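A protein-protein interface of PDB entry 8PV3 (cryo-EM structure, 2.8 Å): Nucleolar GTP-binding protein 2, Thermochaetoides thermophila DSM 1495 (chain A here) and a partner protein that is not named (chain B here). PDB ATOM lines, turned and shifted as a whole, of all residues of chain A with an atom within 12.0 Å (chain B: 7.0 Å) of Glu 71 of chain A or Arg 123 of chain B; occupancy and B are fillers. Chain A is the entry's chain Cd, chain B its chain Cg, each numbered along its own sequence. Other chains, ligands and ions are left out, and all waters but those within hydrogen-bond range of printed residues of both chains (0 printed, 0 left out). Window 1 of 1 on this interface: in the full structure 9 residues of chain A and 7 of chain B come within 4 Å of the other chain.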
ATOM      1  N   LYS A  67      -1.658  -5.487  26.705  1.00  0.00           N
ATOM      2  CA  LYS A  67      -1.463  -4.163  26.127  1.00  0.00           C
ATOM      3  C   LYS A  67      -1.140  -4.336  24.648  1.00  0.00           C
ATOM      4  O   LYS A  67       0.012  -4.594  24.284  1.00  0.00           O
ATOM      5  CB  LYS A  67      -0.346  -3.425  26.858  1.00  0.00           C
ATOM      6  CG  LYS A  67      -0.220  -1.967  26.489  1.00  0.00           C
ATOM      7  CD  LYS A  67      -1.422  -1.196  26.991  1.00  0.00           C
ATOM      8  CE  LYS A  67      -1.461  -1.167  28.508  1.00  0.00           C
ATOM      9  NZ  LYS A  67      -2.629  -0.397  29.017  1.00  0.00           N
ATOM     10  N   ALA A  68      -2.152  -4.190  23.795  1.00  0.00           N
ATOM     11  CA  ALA A  68      -2.026  -4.511  22.375  1.00  0.00           C
ATOM     12  C   ALA A  68      -1.647  -3.251  21.610  1.00  0.00           C
ATOM     13  O   ALA A  68      -2.486  -2.410  21.293  1.00  0.00           O
ATOM     14  CB  ALA A  68      -3.318  -5.121  21.851  1.00  0.00           C
ATOM     15  N   VAL A  69      -0.357  -3.123  21.309  1.00  0.00           N
ATOM     16  CA  VAL A  69       0.196  -1.974  20.605  1.00  0.00           C
ATOM     17  C   VAL A  69       1.149  -2.467  19.524  1.00  0.00           C
ATOM     18  O   VAL A  69       1.719  -3.558  19.636  1.00  0.00           O
ATOM     19  CB  VAL A  69       0.918  -1.014  21.572  1.00  0.00           C
ATOM     20  CG1 VAL A  69      -0.079  -0.257  22.413  1.00  0.00           C
ATOM     21  CG2 VAL A  69       1.832  -1.798  22.482  1.00  0.00           C
ATOM     22  N   ILE A  70       1.316  -1.664  18.476  1.00  0.00           N
ATOM     23  CA  ILE A  70       2.206  -1.971  17.361  1.00  0.00           C
ATOM     24  C   ILE A  70       3.276  -0.891  17.299  1.00  0.00           C
ATOM     25  O   ILE A  70       2.959   0.300  17.191  1.00  0.00           O
ATOM     26  CB  ILE A  70       1.442  -2.060  16.030  1.00  0.00           C
ATOM     27  CG1 ILE A  70       0.406  -3.184  16.072  1.00  0.00           C
ATOM     28  CG2 ILE A  70       2.405  -2.256  14.870  1.00  0.00           C
ATOM     29  CD1 ILE A  70       1.001  -4.568  15.983  1.00  0.00           C
ATOM     30  N   GLU A  71       4.540  -1.302  17.358  1.00  0.00           N
ATOM     31  CA  GLU A  71       5.629  -0.340  17.315  1.00  0.00           C
ATOM     32  C   GLU A  71       5.840   0.178  15.894  1.00  0.00           C
ATOM     33  O   GLU A  71       5.494  -0.496  14.920  1.00  0.00           O
ATOM     34  CB  GLU A  71       6.919  -0.969  17.840  1.00  0.00           C
ATOM     35  CG  GLU A  71       7.740  -1.738  16.818  1.00  0.00           C
ATOM     36  CD  GLU A  71       7.239  -3.152  16.600  1.00  0.00           C
ATOM     37  OE1 GLU A  71       6.294  -3.568  17.301  1.00  0.00           O
ATOM     38  OE2 GLU A  71       7.794  -3.849  15.727  1.00  0.00           O
ATOM     39  N   PRO A  72       6.363   1.395  15.750  1.00  0.00           N
ATOM     40  CA  PRO A  72       6.763   1.860  14.419  1.00  0.00           C
ATOM     41  C   PRO A  72       8.029   1.159  13.955  1.00  0.00           C
ATOM     42  O   PRO A  72       8.998   1.024  14.704  1.00  0.00           O
ATOM     43  CB  PRO A  72       6.987   3.364  14.614  1.00  0.00           C
ATOM     44  CG  PRO A  72       7.185   3.539  16.072  1.00  0.00           C
ATOM     45  CD  PRO A  72       6.366   2.485  16.738  1.00  0.00           C
ATOM     46  N   ASN A  73       8.014   0.716  12.702  1.00  0.00           N
ATOM     47  CA  ASN A  73       9.108  -0.068  12.151  1.00  0.00           C
ATOM     48  C   ASN A  73       9.166   0.168  10.650  1.00  0.00           C
ATOM     49  O   ASN A  73       8.128   0.259   9.993  1.00  0.00           O
ATOM     50  CB  ASN A  73       8.923  -1.559  12.455  1.00  0.00           C
ATOM     51  CG  ASN A  73      10.219  -2.337  12.400  1.00  0.00           C
ATOM     52  OD1 ASN A  73      11.066  -2.101  11.542  1.00  0.00           O
ATOM     53  ND2 ASN A  73      10.377  -3.280  13.319  1.00  0.00           N
ATOM     54  N   ARG A  74      10.386   0.253  10.117  1.00  0.00           N
ATOM     55  CA  ARG A  74      10.548   0.469   8.684  1.00  0.00           C
ATOM     56  C   ARG A  74      10.253  -0.794   7.887  1.00  0.00           C
ATOM     57  O   ARG A  74      10.072  -0.727   6.668  1.00  0.00           O
ATOM     58  CB  ARG A  74      11.961   0.967   8.383  1.00  0.00           C
ATOM     59  N   LYS A  75      10.196  -1.950   8.554  1.00  0.00           N
ATOM     60  CA  LYS A  75       9.947  -3.202   7.851  1.00  0.00           C
ATOM     61  C   LYS A  75       8.500  -3.321   7.392  1.00  0.00           C
ATOM     62  O   LYS A  75       8.192  -4.147   6.525  1.00  0.00           O
ATOM     63  CB  LYS A  75      10.316  -4.389   8.745  1.00  0.00           C
ATOM     64  CG  LYS A  75       9.261  -4.726   9.781  1.00  0.00           C
ATOM     65  CD  LYS A  75       9.314  -6.179  10.209  1.00  0.00           C
ATOM     66  CE  LYS A  75      10.486  -6.442  11.123  1.00  0.00           C
ATOM     67  NZ  LYS A  75      10.416  -7.807  11.708  1.00  0.00           N
ATOM     68  N   TRP A  76       7.597  -2.518   7.959  1.00  0.00           N
ATOM     69  CA  TRP A  76       6.198  -2.592   7.563  1.00  0.00           C
ATOM     70  C   TRP A  76       5.947  -1.976   6.196  1.00  0.00           C
ATOM     71  O   TRP A  76       4.948  -2.314   5.553  1.00  0.00           O
ATOM     72  CB  TRP A  76       5.302  -1.894   8.591  1.00  0.00           C
ATOM     73  CG  TRP A  76       5.434  -2.334  10.031  1.00  0.00           C
ATOM     74  CD1 TRP A  76       5.544  -1.513  11.114  1.00  0.00           C
ATOM     75  CD2 TRP A  76       5.423  -3.676  10.548  1.00  0.00           C
ATOM     76  NE1 TRP A  76       5.622  -2.252  12.266  1.00  0.00           N
ATOM     77  CE2 TRP A  76       5.549  -3.582  11.947  1.00  0.00           C
ATOM     78  CE3 TRP A  76       5.327  -4.944   9.968  1.00  0.00           C
ATOM     79  CZ2 TRP A  76       5.585  -4.702  12.768  1.00  0.00           C
ATOM     80  CZ3 TRP A  76       5.366  -6.051  10.785  1.00  0.00           C
ATOM     81  CH2 TRP A  76       5.491  -5.925  12.169  1.00  0.00           C
ATOM     82  N   PHE A  77       6.826  -1.088   5.736  1.00  0.00           N
ATOM     83  CA  PHE A  77       6.600  -0.319   4.520  1.00  0.00           C
ATOM     84  C   PHE A  77       7.500  -0.767   3.375  1.00  0.00           C
ATOM     85  O   PHE A  77       7.654  -0.039   2.391  1.00  0.00           O
ATOM     86  CB  PHE A  77       6.787   1.171   4.802  1.00  0.00           C
ATOM     87  CG  PHE A  77       5.805   1.725   5.794  1.00  0.00           C
ATOM     88  CD1 PHE A  77       6.071   1.691   7.151  1.00  0.00           C
ATOM     89  CD2 PHE A  77       4.609   2.273   5.369  1.00  0.00           C
ATOM     90  CE1 PHE A  77       5.166   2.190   8.062  1.00  0.00           C
ATOM     91  CE2 PHE A  77       3.701   2.778   6.277  1.00  0.00           C
ATOM     92  CZ  PHE A  77       3.981   2.735   7.624  1.00  0.00           C
ATOM     93  N   THR A  78       8.091  -1.951   3.480  1.00  0.00           N
ATOM     94  CA  THR A  78       8.940  -2.511   2.443  1.00  0.00           C
ATOM     95  C   THR A  78       8.273  -3.726   1.811  1.00  0.00           C
ATOM     96  O   THR A  78       7.336  -4.312   2.356  1.00  0.00           O
ATOM     97  CB  THR A  78      10.311  -2.901   3.006  1.00  0.00           C
ATOM     98  OG1 THR A  78      10.154  -3.961   3.956  1.00  0.00           O
ATOM     99  CG2 THR A  78      10.975  -1.713   3.674  1.00  0.00           C
ATOM    100  N   LYS B 117      15.614 -18.452  22.133  1.00  0.00           N
ATOM    101  CA  LYS B 117      14.631 -17.387  22.018  1.00  0.00           C
ATOM    102  C   LYS B 117      14.525 -16.907  20.578  1.00  0.00           C
ATOM    103  O   LYS B 117      15.517 -16.828  19.851  1.00  0.00           O
ATOM    104  CB  LYS B 117      15.006 -16.219  22.930  1.00  0.00           C
ATOM    105  CG  LYS B 117      14.818 -16.501  24.407  1.00  0.00           C
ATOM    106  CD  LYS B 117      15.781 -15.691  25.254  1.00  0.00           C
ATOM    107  CE  LYS B 117      15.668 -14.209  24.965  1.00  0.00           C
ATOM    108  NZ  LYS B 117      16.769 -13.446  25.611  1.00  0.00           N
ATOM    109  N   THR B 118      13.303 -16.585  20.165  1.00  0.00           N
ATOM    110  CA  THR B 118      13.090 -16.090  18.816  1.00  0.00           C
ATOM    111  C   THR B 118      13.574 -14.651  18.692  1.00  0.00           C
ATOM    112  O   THR B 118      13.733 -13.934  19.685  1.00  0.00           O
ATOM    113  CB  THR B 118      11.617 -16.187  18.426  1.00  0.00           C
ATOM    114  OG1 THR B 118      10.847 -15.284  19.224  1.00  0.00           O
ATOM    115  CG2 THR B 118      11.106 -17.597  18.634  1.00  0.00           C
ATOM    116  N   ARG B 119      13.822 -14.240  17.446  1.00  0.00           N
ATOM    117  CA  ARG B 119      14.377 -12.916  17.190  1.00  0.00           C
ATOM    118  C   ARG B 119      13.393 -11.811  17.544  1.00  0.00           C
ATOM    119  O   ARG B 119      13.808 -10.696  17.872  1.00  0.00           O
ATOM    120  CB  ARG B 119      14.806 -12.806  15.730  1.00  0.00           C
ATOM    121  CG  ARG B 119      15.854 -13.819  15.325  1.00  0.00           C
ATOM    122  CD  ARG B 119      16.270 -13.630  13.883  1.00  0.00           C
ATOM    123  NE  ARG B 119      17.099 -12.445  13.713  1.00  0.00           N
ATOM    124  CZ  ARG B 119      18.423 -12.461  13.665  1.00  0.00           C
ATOM    125  NH1 ARG B 119      19.104 -13.591  13.746  1.00  0.00           N
ATOM    126  NH2 ARG B 119      19.080 -11.314  13.527  1.00  0.00           N
ATOM    127  N   GLU B 120      12.091 -12.094  17.478  1.00  0.00           N
ATOM    128  CA  GLU B 120      11.106 -11.115  17.921  1.00  0.00           C
ATOM    129  C   GLU B 120      11.036 -11.061  19.440  1.00  0.00           C
ATOM    130  O   GLU B 120      10.800  -9.994  20.020  1.00  0.00           O
ATOM    131  CB  GLU B 120       9.727 -11.433  17.332  1.00  0.00           C
ATOM    132  CG  GLU B 120       9.580 -11.233  15.816  1.00  0.00           C
ATOM    133  CD  GLU B 120      10.297 -12.278  14.969  1.00  0.00           C
ATOM    134  OE1 GLU B 120      10.751 -13.303  15.521  1.00  0.00           O
ATOM    135  OE2 GLU B 120      10.410 -12.067  13.742  1.00  0.00           O
ATOM    136  N   GLN B 121      11.230 -12.203  20.101  1.00  0.00           N
ATOM    137  CA  GLN B 121      11.218 -12.249  21.557  1.00  0.00           C
ATOM    138  C   GLN B 121      12.424 -11.551  22.166  1.00  0.00           C
ATOM    139  O   GLN B 121      12.291 -10.907  23.213  1.00  0.00           O
ATOM    140  CB  GLN B 121      11.158 -13.705  22.021  1.00  0.00           C
ATOM    141  CG  GLN B 121      11.179 -13.922  23.521  1.00  0.00           C
ATOM    142  CD  GLN B 121      11.221 -15.392  23.887  1.00  0.00           C
ATOM    143  OE1 GLN B 121      11.181 -16.259  23.016  1.00  0.00           O
ATOM    144  NE2 GLN B 121      11.306 -15.678  25.179  1.00  0.00           N
ATOM    145  N   ARG B 122      13.589 -11.639  21.530  1.00  0.00           N
ATOM    146  CA  ARG B 122      14.822 -11.115  22.101  1.00  0.00           C
ATOM    147  C   ARG B 122      15.139  -9.690  21.654  1.00  0.00           C
ATOM    148  O   ARG B 122      16.274  -9.237  21.839  1.00  0.00           O
ATOM    149  CB  ARG B 122      15.991 -12.045  21.768  1.00  0.00           C
ATOM    150  CG  ARG B 122      16.400 -12.058  20.307  1.00  0.00           C
ATOM    151  CD  ARG B 122      17.237 -13.278  19.983  1.00  0.00           C
ATOM    152  NE  ARG B 122      18.036 -13.081  18.780  1.00  0.00           N
ATOM    153  CZ  ARG B 122      18.723 -14.037  18.173  1.00  0.00           C
ATOM    154  NH1 ARG B 122      18.720 -15.281  18.624  1.00  0.00           N
ATOM    155  NH2 ARG B 122      19.428 -13.740  17.087  1.00  0.00           N
ATOM    156  N   ARG B 123      14.171  -8.972  21.087  1.00  0.00           N
ATOM    157  CA  ARG B 123      14.408  -7.603  20.647  1.00  0.00           C
ATOM    158  C   ARG B 123      14.652  -6.673  21.830  1.00  0.00           C
ATOM    159  O   ARG B 123      14.116  -6.864  22.924  1.00  0.00           O
ATOM    160  CB  ARG B 123      13.226  -7.079  19.833  1.00  0.00           C
ATOM    161  CG  ARG B 123      13.184  -7.568  18.404  1.00  0.00           C
ATOM    162  CD  ARG B 123      12.180  -6.784  17.580  1.00  0.00           C
ATOM    163  NE  ARG B 123      12.493  -5.360  17.553  1.00  0.00           N
ATOM    164  CZ  ARG B 123      11.690  -4.426  17.063  1.00  0.00           C
ATOM    165  NH1 ARG B 123      10.504  -4.727  16.562  1.00  0.00           N
ATOM    166  NH2 ARG B 123      12.090  -3.158  17.073  1.00  0.00           N
ATOM    167  N   ASN B 124      15.478  -5.652  21.596  1.00  0.00           N
ATOM    168  CA  ASN B 124      15.745  -4.619  22.596  1.00  0.00           C
ATOM    169  C   ASN B 124      14.723  -3.494  22.432  1.00  0.00           C
ATOM    170  O   ASN B 124      15.036  -2.357  22.075  1.00  0.00           O
ATOM    171  CB  ASN B 124      17.171  -4.104  22.471  1.00  0.00           C
ATOM    172  CG  ASN B 124      17.572  -3.209  23.626  1.00  0.00           C
ATOM    173  OD1 ASN B 124      16.870  -3.121  24.631  1.00  0.00           O
ATOM    174  ND2 ASN B 124      18.708  -2.538  23.487  1.00  0.00           N
ATOM    175  N   LEU B 125      13.467  -3.840  22.698  1.00  0.00           N
ATOM    176  CA  LEU B 125      12.379  -2.881  22.624  1.00  0.00           C
ATOM    177  C   LEU B 125      11.245  -3.376  23.502  1.00  0.00           C
ATOM    178  O   LEU B 125      10.960  -4.574  23.537  1.00  0.00           O
ATOM    179  CB  LEU B 125      11.888  -2.689  21.184  1.00  0.00           C
ATOM    180  CG  LEU B 125      11.068  -1.425  20.927  1.00  0.00           C
ATOM    181  CD1 LEU B 125      11.923  -0.185  21.123  1.00  0.00           C
ATOM    182  CD2 LEU B 125      10.450  -1.445  19.542  1.00  0.00           C
ATOM    183  N   GLN B 126      10.605  -2.449  24.205  1.00  0.00           N
ATOM    184  CA  GLN B 126       9.446  -2.783  25.016  1.00  0.00           C
ATOM    185  C   GLN B 126       8.546  -1.564  25.084  1.00  0.00           C
ATOM    186  O   GLN B 126       8.986  -0.438  24.840  1.00  0.00           O
ATOM    187  CB  GLN B 126       9.847  -3.239  26.422  1.00  0.00           C
ATOM    188  CG  GLN B 126      10.365  -2.131  27.316  1.00  0.00           C
ATOM    189  CD  GLN B 126      10.658  -2.613  28.719  1.00  0.00           C
ATOM    190  OE1 GLN B 126      10.795  -3.811  28.958  1.00  0.00           O
ATOM    191  NE2 GLN B 126      10.747  -1.681  29.658  1.00  0.00           N
ATOM    192  N   TRP B 134       7.484   3.694  23.525  1.00  0.00           N
ATOM    193  CA  TRP B 134       8.360   2.562  23.271  1.00  0.00           C
ATOM    194  C   TRP B 134       9.774   2.893  23.723  1.00  0.00           C
ATOM    195  O   TRP B 134      10.309   3.958  23.402  1.00  0.00           O
ATOM    196  CB  TRP B 134       8.358   2.193  21.788  1.00  0.00           C
ATOM    197  CG  TRP B 134       7.100   1.533  21.348  1.00  0.00           C
ATOM    198  CD1 TRP B 134       6.005   2.135  20.809  1.00  0.00           C
ATOM    199  CD2 TRP B 134       6.802   0.136  21.409  1.00  0.00           C
ATOM    200  NE1 TRP B 134       5.041   1.201  20.531  1.00  0.00           N
ATOM    201  CE2 TRP B 134       5.506  -0.035  20.893  1.00  0.00           C
ATOM    202  CE3 TRP B 134       7.505  -0.986  21.853  1.00  0.00           C
ATOM    203  CZ2 TRP B 134       4.901  -1.282  20.803  1.00  0.00           C
ATOM    204  CZ3 TRP B 134       6.901  -2.224  21.767  1.00  0.00           C
ATOM    205  CH2 TRP B 134       5.611  -2.362  21.248  1.00  0.00           C
ATOM    206  N   LYS B 137      15.105  -2.031  26.522  1.00  0.00           N
ATOM    207  CA  LYS B 137      15.331  -2.742  27.774  1.00  0.00           C
ATOM    208  C   LYS B 137      16.707  -2.452  28.357  1.00  0.00           C
ATOM    209  O   LYS B 137      16.849  -2.360  29.580  1.00  0.00           O
ATOM    210  CB  LYS B 137      15.162  -4.247  27.569  1.00  0.00           C
ATOM    211  CG  LYS B 137      13.894  -4.642  26.844  1.00  0.00           C
ATOM    212  CD  LYS B 137      13.899  -6.120  26.505  1.00  0.00           C
ATOM    213  CE  LYS B 137      12.568  -6.556  25.921  1.00  0.00           C
ATOM    214  NZ  LYS B 137      12.602  -7.974  25.475  1.00  0.00           N
ATOM    215  N   TRP B 138      17.722  -2.312  27.509  1.00  0.00           N
ATOM    216  CA  TRP B 138      19.088  -2.096  27.957  1.00  0.00           C
ATOM    217  C   TRP B 138      19.754  -1.097  27.023  1.00  0.00           C
ATOM    218  O   TRP B 138      19.140  -0.595  26.079  1.00  0.00           O
ATOM    219  CB  TRP B 138      19.870  -3.416  28.012  1.00  0.00           C
ATOM    220  CG  TRP B 138      19.977  -4.101  26.688  1.00  0.00           C
ATOM    221  CD1 TRP B 138      19.060  -4.936  26.129  1.00  0.00           C
ATOM    222  CD2 TRP B 138      21.062  -4.018  25.758  1.00  0.00           C
ATOM    223  NE1 TRP B 138      19.502  -5.377  24.909  1.00  0.00           N
ATOM    224  CE2 TRP B 138      20.729  -4.827  24.657  1.00  0.00           C
ATOM    225  CE3 TRP B 138      22.285  -3.343  25.752  1.00  0.00           C
ATOM    226  CZ2 TRP B 138      21.568  -4.972  23.560  1.00  0.00           C
ATOM    227  CZ3 TRP B 138      23.117  -3.489  24.662  1.00  0.00           C
ATOM    228  CH2 TRP B 138      22.756  -4.298  23.581  1.00  0.00           C
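The guanidinium group of Arg 123 of chain B is in salt-bridge range of the side-chain carboxylate of Glu 71 of chain A, 3.0 Å away.
The indole nitrogen (NE1) of Trp 76 of chain A sits at hydrogen-bond distance from the backbone carbonyl oxygen (O) of Glu 71 of chain A, at 3.2 Å.
The side-chain amide oxygen (OD1) of Asn 73 of chain A sits at hydrogen-bond distance from the backbone NH (N) of Lys 75 of chain A (3.1 Å).
The side-chain amino group of Lys 137 of chain B sits at hydrogen-bond distance from the backbone carbonyl oxygen of Arg 123 of chain B (3.2 Å).
Val 69 of chain A touches Trp 134 of chain B (CG2 to CZ2, 3.5 Å).
C of Ile 70 of chain A touches CZ2 of Trp 134 of chain B, at 3.9 Å.
Glu 71 of chain A touches Leu 125 of chain B (CG to CD2, 3.9 Å).
CZ2 of Trp 134 of chain B touches N of Glu 71 of chain A, at 3.5 Å.
NH1 of Arg 123 of chain B touches ND2 of Asn 73 of chain A (3.6 Å).
Of chain B, only Arg 123, Leu 125 and Trp 134 come within 4 Å of Glu 71 of chain A.
Of chain A, only Glu 71 (3.0 Å) and Asn 73 (3.6 Å) come within 4 Å of Arg 123 of chain B.
No residue of chain A comes within 4 Å of Glu 120 of chain B.
No residue of chain A comes within 4 Å of Asn 124 of chain B.
Leu 125 of chain B touches just one residue of chain A: Glu 71 (3.9 Å).
Printed residues of chain B within 4 Å of Ile 70 of chain A: Trp 134 (3.9 Å).
Of the printed residues of chain B, Val 69 of chain A touches Trp 134 (3.5 Å).
Of the printed residues of chain A, Trp 134 of chain B touches Val 69, Ile 70 and Glu 71.
Printed residues of chain B within 4 Å of Asn 73 of chain A: Arg 123.
The nearest printed residue of chain B that does not touch Glu 71 of chain A is Gln 126 of chain B (7.3 Å).
The nearest printed residue of chain B that does not touch Asn 73 of chain A is Leu 125 of chain B (6.5 Å).
Hydrophobic or aromatic side chains of chain B within 4 Å of the printed part of chain A: Leu 125 and Trp 134.
Of the 12 printed residues of chain A, 4 touch a printed residue of chain B.
Hydrophobic or aromatic side chains of chain A that line the printed part of chain B: Val 69.
Among the printed residues, Asp or Glu carboxylates within 4 Å of a Lys or Arg side-chain nitrogen of the other chain: Glu 71 of chain A with Arg 123 of chain B (3.0 Å).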
